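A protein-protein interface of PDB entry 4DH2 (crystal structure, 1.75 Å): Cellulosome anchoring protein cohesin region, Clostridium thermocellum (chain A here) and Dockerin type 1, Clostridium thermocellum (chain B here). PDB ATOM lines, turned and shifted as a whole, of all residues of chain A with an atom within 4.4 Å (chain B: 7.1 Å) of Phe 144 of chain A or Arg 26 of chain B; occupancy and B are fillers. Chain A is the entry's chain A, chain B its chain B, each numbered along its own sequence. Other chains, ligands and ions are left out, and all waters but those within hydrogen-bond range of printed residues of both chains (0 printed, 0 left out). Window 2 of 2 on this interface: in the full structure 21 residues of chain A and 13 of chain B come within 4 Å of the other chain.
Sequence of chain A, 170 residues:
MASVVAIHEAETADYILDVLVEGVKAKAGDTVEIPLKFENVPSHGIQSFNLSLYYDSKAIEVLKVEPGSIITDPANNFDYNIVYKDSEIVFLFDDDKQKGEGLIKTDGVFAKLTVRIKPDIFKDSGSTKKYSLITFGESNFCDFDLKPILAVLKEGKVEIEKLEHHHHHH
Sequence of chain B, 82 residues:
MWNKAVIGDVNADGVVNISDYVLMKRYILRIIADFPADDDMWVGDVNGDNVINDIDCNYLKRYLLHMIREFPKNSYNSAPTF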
ATOM      1  N   GLY A  45     -11.108  21.137  15.607  1.00  0.00           N
ATOM      2  CA  GLY A  45     -11.074  20.200  14.501  1.00  0.00           C
ATOM      3  C   GLY A  45     -11.143  20.765  13.095  1.00  0.00           C
ATOM      4  O   GLY A  45     -11.832  21.751  12.826  1.00  0.00           O
ATOM      5  N   GLN A  47     -12.483  20.161   9.408  1.00  0.00           N
ATOM      6  CA  GLN A  47     -13.516  19.533   8.589  1.00  0.00           C
ATOM      7  C   GLN A  47     -12.993  19.109   7.228  1.00  0.00           C
ATOM      8  O   GLN A  47     -13.314  18.016   6.713  1.00  0.00           O
ATOM      9  CB  GLN A  47     -14.661  20.534   8.414  1.00  0.00           C
ATOM     10  CG  GLN A  47     -15.654  20.220   7.307  1.00  0.00           C
ATOM     11  CD  GLN A  47     -16.551  19.061   7.688  1.00  0.00           C
ATOM     12  OE1 GLN A  47     -17.141  19.054   8.763  1.00  0.00           O
ATOM     13  NE2 GLN A  47     -16.619  18.061   6.830  1.00  0.00           N
ATOM     14  N   GLN A  98     -20.436  14.769   7.585  1.00  0.00           N
ATOM     15  CA  GLN A  98     -20.873  16.114   7.917  1.00  0.00           C
ATOM     16  C   GLN A  98     -21.627  16.270   9.214  1.00  0.00           C
ATOM     17  O   GLN A  98     -22.486  17.141   9.302  1.00  0.00           O
ATOM     18  CB  GLN A  98     -21.737  16.694   6.810  1.00  0.00           C
ATOM     19  CG  GLN A  98     -21.086  16.638   5.436  1.00  0.00           C
ATOM     20  CD  GLN A  98     -19.831  17.491   5.350  1.00  0.00           C
ATOM     21  OE1 GLN A  98     -19.674  18.473   6.081  1.00  0.00           O
ATOM     22  NE2 GLN A  98     -18.925  17.115   4.448  1.00  0.00           N
ATOM     23  N   LYS A  99     -21.237  15.507  10.231  1.00  0.00           N
ATOM     24  CA  LYS A  99     -21.888  15.564  11.519  1.00  0.00           C
ATOM     25  C   LYS A  99     -20.863  15.861  12.593  1.00  0.00           C
ATOM     26  O   LYS A  99     -21.136  15.669  13.768  1.00  0.00           O
ATOM     27  CB  LYS A  99     -22.580  14.225  11.826  1.00  0.00           C
ATOM     28  CG  LYS A  99     -23.713  13.907  10.865  1.00  0.00           C
ATOM     29  CD  LYS A  99     -24.605  12.784  11.367  1.00  0.00           C
ATOM     30  CE  LYS A  99     -25.845  12.653  10.485  1.00  0.00           C
ATOM     31  NZ  LYS A  99     -26.772  11.593  10.985  1.00  0.00           N
ATOM     32  N   GLY A 100     -19.672  16.306  12.198  1.00  0.00           N
ATOM     33  CA  GLY A 100     -18.697  16.738  13.179  1.00  0.00           C
ATOM     34  C   GLY A 100     -18.089  15.606  13.993  1.00  0.00           C
ATOM     35  O   GLY A 100     -17.542  15.844  15.071  1.00  0.00           O
ATOM     36  N   ASP A 143     -12.823  24.660   9.297  1.00  0.00           N
ATOM     37  CA  ASP A 143     -13.471  23.945  10.376  1.00  0.00           C
ATOM     38  C   ASP A 143     -14.897  23.576  10.002  1.00  0.00           C
ATOM     39  O   ASP A 143     -15.324  23.800   8.866  1.00  0.00           O
ATOM     40  CB  ASP A 143     -13.399  24.685  11.716  1.00  0.00           C
ATOM     41  CG  ASP A 143     -14.266  25.898  11.804  1.00  0.00           C
ATOM     42  OD1 ASP A 143     -15.120  26.155  10.930  1.00  0.00           O
ATOM     43  OD2 ASP A 143     -14.105  26.598  12.849  1.00  0.00           O
ATOM     44  N   PHE A 144     -15.592  22.979  10.957  1.00  0.00           N
ATOM     45  CA  PHE A 144     -16.961  22.508  10.712  1.00  0.00           C
ATOM     46  C   PHE A 144     -17.878  23.628  10.236  1.00  0.00           C
ATOM     47  O   PHE A 144     -18.759  23.421   9.376  1.00  0.00           O
ATOM     48  CB  PHE A 144     -17.552  21.885  11.960  1.00  0.00           C
ATOM     49  CG  PHE A 144     -18.940  21.393  11.737  1.00  0.00           C
ATOM     50  CD1 PHE A 144     -19.144  20.170  11.154  1.00  0.00           C
ATOM     51  CD2 PHE A 144     -20.028  22.168  12.091  1.00  0.00           C
ATOM     52  CE1 PHE A 144     -20.435  19.705  10.938  1.00  0.00           C
ATOM     53  CE2 PHE A 144     -21.303  21.715  11.876  1.00  0.00           C
ATOM     54  CZ  PHE A 144     -21.500  20.481  11.296  1.00  0.00           C
ATOM     55  N   ASP A 145     -17.653  24.840  10.754  1.00  0.00           N
ATOM     56  CA  ASP A 145     -18.437  25.993  10.358  1.00  0.00           C
ATOM     57  C   ASP A 145     -17.932  26.728   9.134  1.00  0.00           C
ATOM     58  O   ASP A 145     -18.427  27.812   8.812  1.00  0.00           O
ATOM     59  CB  ASP A 145     -18.546  26.974  11.533  1.00  0.00           C
ATOM     60  CG  ASP A 145     -19.234  26.356  12.730  1.00  0.00           C
ATOM     61  OD1 ASP A 145     -20.364  25.814  12.556  1.00  0.00           O
ATOM     62  OD2 ASP A 145     -18.641  26.360  13.834  1.00  0.00           O
ATOM     63  N   LEU A 146     -16.987  26.104   8.433  1.00  0.00           N
ATOM     64  CA  LEU A 146     -16.374  26.635   7.212  1.00  0.00           C
ATOM     65  C   LEU A 146     -15.511  27.860   7.474  1.00  0.00           C
ATOM     66  O   LEU A 146     -15.160  28.602   6.537  1.00  0.00           O
ATOM     67  CB  LEU A 146     -17.411  26.973   6.138  1.00  0.00           C
ATOM     68  CG  LEU A 146     -18.457  25.867   5.905  1.00  0.00           C
ATOM     69  CD1 LEU A 146     -19.426  26.261   4.802  1.00  0.00           C
ATOM     70  CD2 LEU A 146     -17.775  24.579   5.587  1.00  0.00           C
ATOM     71  N   ASP B  20     -16.917  25.112  -1.033  1.00  0.00           N
ATOM     72  CA  ASP B  20     -17.963  24.743  -1.971  1.00  0.00           C
ATOM     73  C   ASP B  20     -18.206  23.245  -1.963  1.00  0.00           C
ATOM     74  O   ASP B  20     -19.331  22.780  -2.130  1.00  0.00           O
ATOM     75  CB  ASP B  20     -17.578  25.189  -3.361  1.00  0.00           C
ATOM     76  CG  ASP B  20     -17.339  26.686  -3.410  1.00  0.00           C
ATOM     77  OD1 ASP B  20     -18.310  27.450  -3.301  1.00  0.00           O
ATOM     78  OD2 ASP B  20     -16.160  27.060  -3.492  1.00  0.00           O
ATOM     79  N   TYR B  21     -17.138  22.483  -1.789  1.00  0.00           N
ATOM     80  CA  TYR B  21     -17.256  21.026  -1.700  1.00  0.00           C
ATOM     81  C   TYR B  21     -18.051  20.587  -0.466  1.00  0.00           C
ATOM     82  O   TYR B  21     -18.965  19.740  -0.544  1.00  0.00           O
ATOM     83  CB  TYR B  21     -15.848  20.420  -1.644  1.00  0.00           C
ATOM     84  CG  TYR B  21     -15.774  18.911  -1.708  1.00  0.00           C
ATOM     85  CD1 TYR B  21     -16.339  18.209  -2.759  1.00  0.00           C
ATOM     86  CD2 TYR B  21     -15.086  18.199  -0.734  1.00  0.00           C
ATOM     87  CE1 TYR B  21     -16.264  16.842  -2.818  1.00  0.00           C
ATOM     88  CE2 TYR B  21     -15.003  16.815  -0.790  1.00  0.00           C
ATOM     89  CZ  TYR B  21     -15.600  16.155  -1.844  1.00  0.00           C
ATOM     90  OH  TYR B  21     -15.532  14.787  -1.930  1.00  0.00           O
ATOM     91  N   VAL B  22     -17.700  21.141   0.685  1.00  0.00           N
ATOM     92  CA  VAL B  22     -18.413  20.829   1.918  1.00  0.00           C
ATOM     93  C   VAL B  22     -19.877  21.244   1.814  1.00  0.00           C
ATOM     94  O   VAL B  22     -20.789  20.462   2.188  1.00  0.00           O
ATOM     95  CB  VAL B  22     -17.752  21.544   3.108  1.00  0.00           C
ATOM     96  CG1 VAL B  22     -18.560  21.346   4.357  1.00  0.00           C
ATOM     97  CG2 VAL B  22     -16.305  20.993   3.313  1.00  0.00           C
ATOM     98  N   LEU B  23     -20.131  22.440   1.265  1.00  0.00           N
ATOM     99  CA  LEU B  23     -21.506  22.894   1.070  1.00  0.00           C
ATOM    100  C   LEU B  23     -22.302  21.983   0.120  1.00  0.00           C
ATOM    101  O   LEU B  23     -23.478  21.659   0.387  1.00  0.00           O
ATOM    102  CB  LEU B  23     -21.546  24.341   0.581  1.00  0.00           C
ATOM    103  CG  LEU B  23     -21.198  25.406   1.631  1.00  0.00           C
ATOM    104  CD1 LEU B  23     -21.036  26.748   0.944  1.00  0.00           C
ATOM    105  CD2 LEU B  23     -22.230  25.507   2.735  1.00  0.00           C
ATOM    106  N   MET B  24     -21.692  21.565  -0.976  1.00  0.00           N
ATOM    107  CA  MET B  24     -22.340  20.650  -1.899  1.00  0.00           C
ATOM    108  C   MET B  24     -22.738  19.350  -1.180  1.00  0.00           C
ATOM    109  O   MET B  24     -23.868  18.859  -1.315  1.00  0.00           O
ATOM    110  CB  MET B  24     -21.390  20.329  -3.048  1.00  0.00           C
ATOM    111  CG  MET B  24     -21.884  19.237  -3.953  1.00  0.00           C
ATOM    112  SD  MET B  24     -23.237  19.771  -4.998  1.00  0.00           S
ATOM    113  CE  MET B  24     -22.207  20.497  -6.283  1.00  0.00           C
ATOM    114  N   LYS B  25     -21.789  18.774  -0.445  1.00  0.00           N
ATOM    115  CA  LYS B  25     -22.062  17.560   0.334  1.00  0.00           C
ATOM    116  C   LYS B  25     -23.206  17.749   1.301  1.00  0.00           C
ATOM    117  O   LYS B  25     -24.116  16.878   1.390  1.00  0.00           O
ATOM    118  CB  LYS B  25     -20.810  17.083   1.082  1.00  0.00           C
ATOM    119  CG  LYS B  25     -19.865  16.240   0.232  1.00  0.00           C
ATOM    120  CD  LYS B  25     -18.878  15.482   1.127  1.00  0.00           C
ATOM    121  CE  LYS B  25     -17.780  14.700   0.360  1.00  0.00           C
ATOM    122  NZ  LYS B  25     -16.679  14.105   1.275  1.00  0.00           N
ATOM    123  N   ARG B  26     -23.186  18.845   2.055  1.00  0.00           N
ATOM    124  CA  ARG B  26     -24.264  19.096   3.017  1.00  0.00           C
ATOM    125  C   ARG B  26     -25.572  19.332   2.325  1.00  0.00           C
ATOM    126  O   ARG B  26     -26.615  18.937   2.809  1.00  0.00           O
ATOM    127  CB  ARG B  26     -23.918  20.304   3.890  1.00  0.00           C
ATOM    128  CG  ARG B  26     -22.764  19.970   4.812  1.00  0.00           C
ATOM    129  CD  ARG B  26     -22.366  21.172   5.694  1.00  0.00           C
ATOM    130  NE  ARG B  26     -21.197  20.781   6.455  1.00  0.00           N
ATOM    131  CZ  ARG B  26     -20.510  21.586   7.256  1.00  0.00           C
ATOM    132  NH1 ARG B  26     -20.920  22.827   7.430  1.00  0.00           N
ATOM    133  NH2 ARG B  26     -19.434  21.132   7.877  1.00  0.00           N
ATOM    134  N   TYR B  27     -25.523  19.980   1.175  1.00  0.00           N
ATOM    135  CA  TYR B  27     -26.740  20.243   0.446  1.00  0.00           C
ATOM    136  C   TYR B  27     -27.379  18.942  -0.055  1.00  0.00           C
ATOM    137  O   TYR B  27     -28.589  18.759   0.109  1.00  0.00           O
ATOM    138  CB  TYR B  27     -26.436  21.200  -0.698  1.00  0.00           C
ATOM    139  CG  TYR B  27     -27.555  21.432  -1.680  1.00  0.00           C
ATOM    140  CD1 TYR B  27     -28.288  22.613  -1.652  1.00  0.00           C
ATOM    141  CD2 TYR B  27     -27.807  20.521  -2.688  1.00  0.00           C
ATOM    142  CE1 TYR B  27     -29.283  22.859  -2.573  1.00  0.00           C
ATOM    143  CE2 TYR B  27     -28.818  20.743  -3.605  1.00  0.00           C
ATOM    144  CZ  TYR B  27     -29.556  21.918  -3.551  1.00  0.00           C
ATOM    145  OH  TYR B  27     -30.553  22.169  -4.490  1.00  0.00           O
ATOM    146  N   ILE B  28     -26.579  18.051  -0.622  1.00  0.00           N
ATOM    147  CA  ILE B  28     -27.122  16.778  -1.133  1.00  0.00           C
ATOM    148  C   ILE B  28     -27.630  15.923   0.021  1.00  0.00           C
ATOM    149  O   ILE B  28     -28.608  15.191  -0.132  1.00  0.00           O
ATOM    150  CB  ILE B  28     -26.111  16.039  -2.005  1.00  0.00           C
ATOM    151  CG1 ILE B  28     -25.826  16.857  -3.267  1.00  0.00           C
ATOM    152  CG2 ILE B  28     -26.637  14.652  -2.404  1.00  0.00           C
ATOM    153  CD1 ILE B  28     -24.547  16.438  -3.925  1.00  0.00           C
ATOM    154  N   LEU B  29     -27.012  16.045   1.193  1.00  0.00           N
ATOM    155  CA  LEU B  29     -27.466  15.310   2.370  1.00  0.00           C
ATOM    156  C   LEU B  29     -28.666  15.940   3.028  1.00  0.00           C
ATOM    157  O   LEU B  29     -29.242  15.380   3.954  1.00  0.00           O
ATOM    158  CB  LEU B  29     -26.347  15.206   3.401  1.00  0.00           C
ATOM    159  CG  LEU B  29     -25.188  14.328   3.003  1.00  0.00           C
ATOM    160  CD1 LEU B  29     -24.020  14.541   3.969  1.00  0.00           C
ATOM    161  CD2 LEU B  29     -25.639  12.863   3.023  1.00  0.00           C
ATOM    162  N   ARG B  30     -29.014  17.124   2.563  1.00  0.00           N
ATOM    163  CA  ARG B  30     -30.069  17.941   3.131  1.00  0.00           C
ATOM    164  C   ARG B  30     -29.708  18.339   4.558  1.00  0.00           C
ATOM    165  O   ARG B  30     -30.563  18.624   5.387  1.00  0.00           O
ATOM    166  CB  ARG B  30     -31.432  17.209   3.036  1.00  0.00           C
ATOM    167  CG  ARG B  30     -32.623  18.028   3.429  1.00  0.00           C
ATOM    168  CD  ARG B  30     -32.599  19.403   2.841  1.00  0.00           C
ATOM    169  NE  ARG B  30     -33.713  20.225   3.311  1.00  0.00           N
ATOM    170  CZ  ARG B  30     -33.731  20.897   4.458  1.00  0.00           C
ATOM    171  NH1 ARG B  30     -32.696  20.845   5.307  1.00  0.00           N
ATOM    172  NH2 ARG B  30     -34.803  21.621   4.761  1.00  0.00           N
ATOM    173  N   ILE B  31     -28.404  18.393   4.832  1.00  0.00           N
ATOM    174  CA  ILE B  31     -27.943  18.993   6.086  1.00  0.00           C
ATOM    175  C   ILE B  31     -28.132  20.504   6.033  1.00  0.00           C
ATOM    176  O   ILE B  31     -28.355  21.155   7.060  1.00  0.00           O
ATOM    177  CB  ILE B  31     -26.488  18.572   6.413  1.00  0.00           C
ATOM    178  CG1 ILE B  31     -26.529  17.162   7.023  1.00  0.00           C
ATOM    179  CG2 ILE B  31     -25.860  19.571   7.392  1.00  0.00           C
ATOM    180  CD1 ILE B  31     -25.282  16.438   7.028  1.00  0.00           C
ATOM    181  N   ILE B  32     -28.070  21.066   4.823  1.00  0.00           N
ATOM    182  CA  ILE B  32     -28.580  22.413   4.573  1.00  0.00           C
ATOM    183  C   ILE B  32     -29.653  22.324   3.490  1.00  0.00           C
ATOM    184  O   ILE B  32     -29.643  21.417   2.646  1.00  0.00           O
ATOM    185  CB  ILE B  32     -27.479  23.419   4.127  1.00  0.00           C
ATOM    186  CG1 ILE B  32     -26.816  22.938   2.828  1.00  0.00           C
ATOM    187  CG2 ILE B  32     -26.483  23.652   5.281  1.00  0.00           C
ATOM    188  CD1 ILE B  32     -25.690  23.855   2.259  1.00  0.00           C
ATOM    189  N   ALA B  33     -30.573  23.267   3.521  1.00  0.00           N
ATOM    190  CA  ALA B  33     -31.736  23.220   2.647  1.00  0.00           C
ATOM    191  C   ALA B  33     -31.381  23.834   1.316  1.00  0.00           C
ATOM    192  O   ALA B  33     -31.910  23.432   0.286  1.00  0.00           O
ATOM    193  CB  ALA B  33     -32.883  23.972   3.262  1.00  0.00           C
ATOM    194  N   PHE B  35     -28.155  26.417  -1.009  1.00  0.00           N
ATOM    195  CA  PHE B  35     -26.836  27.054  -1.121  1.00  0.00           C
ATOM    196  C   PHE B  35     -26.910  28.534  -0.778  1.00  0.00           C
ATOM    197  O   PHE B  35     -27.954  29.166  -0.953  1.00  0.00           O
ATOM    198  CB  PHE B  35     -26.290  26.919  -2.541  1.00  0.00           C
ATOM    199  CG  PHE B  35     -25.878  25.536  -2.907  1.00  0.00           C
ATOM    200  CD1 PHE B  35     -25.050  24.802  -2.087  1.00  0.00           C
ATOM    201  CD2 PHE B  35     -26.303  24.978  -4.091  1.00  0.00           C
ATOM    202  CE1 PHE B  35     -24.661  23.536  -2.436  1.00  0.00           C
ATOM    203  CE2 PHE B  35     -25.921  23.708  -4.445  1.00  0.00           C
ATOM    204  CZ  PHE B  35     -25.106  22.985  -3.618  1.00  0.00           C
ATOM    205  N   CYS B  57     -20.975  16.531  -7.032  1.00  0.00           N
ATOM    206  CA  CYS B  57     -20.024  16.495  -5.919  1.00  0.00           C
ATOM    207  C   CYS B  57     -18.718  15.841  -6.353  1.00  0.00           C
ATOM    208  O   CYS B  57     -17.627  16.315  -6.034  1.00  0.00           O
ATOM    209  CB  CYS B  57     -20.603  15.710  -4.760  1.00  0.00           C
ATOM    210  SG  CYS B  57     -19.958  16.261  -3.183  1.00  0.00           S
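Of chain B, only Arg 26 comes within 4 Å of Phe 144 of chain A. Printed residues of chain A within 4 Å of Val 22 of chain B: Gln 98 and Leu 146. Printed residues of chain A within 4 Å of Leu 23 of chain B: Leu 146 (3.6 Å). Of the printed residues of chain A, Ile 31 of chain B touches Gln 98. The nearest residue of chain B that does not touch Phe 144 of chain A is Val 22 of chain B (5.4 Å). The nearest residue of chain A that does not touch Arg 26 of chain B is Leu 146 of chain A (4.04 Å).
Among the printed residues, merely in contact across the chains: Gln 98 of chain A with Val 22 of chain B, Leu 146 of chain A with Val 22 of chain B, Gln 98 of chain A with Ile 31 of chain B, Leu 146 of chain A with Leu 23 of chain B, Gln 98 of chain A with Lys 25 of chain B and Gln 98 of chain A with Leu 29 of chain B.
NH2 of Arg 26 of chain B sits at hydrogen-bond distance from OE1 of Gln 47 of chain A (3.2 Å). The guanidinium group (NE) of Arg 26 of chain B sits at hydrogen-bond distance from the side-chain amide oxygen (OE1) of Gln 98 of chain A, 2.8 Å away. The backbone carbonyl oxygen of Phe 144 of chain A lies within hydrogen-bond range of the guanidinium group of Arg 26 of chain B (2.8 Å).
Hydrophobic or aromatic side chains of chain A that line the printed part of chain B: Phe 144 and Leu 146. Hydrophobic or aromatic side chains of chain B that line the printed part of chain A: Val 22, Leu 23, Leu 29 and Ile 31. Among the printed residues, 9 pairs touch across the chains. Among the printed residues, no Asp or Glu carboxylate lies within 4 Å of a Lys or Arg side-chain nitrogen of the other chain.
NE2 of Gln 47 of chain A is in hydrogen-bond range of OE1 of Gln 98 of chain A. The side-chain carboxylate (OD1) of Asp 143 of chain A lies within hydrogen-bond range of the backbone NH (N) of Leu 146 of chain A (3.1 Å). OH of Tyr 21 of chain B sits close to NZ of Lys 25 of chain B (3.5 Å). O of Arg 26 of chain B lies within hydrogen-bond range of N of Ile 31 of chain B (2.8 Å). N of Ile 32 of chain B is in hydrogen-bond range of O of Arg 26 of chain B.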
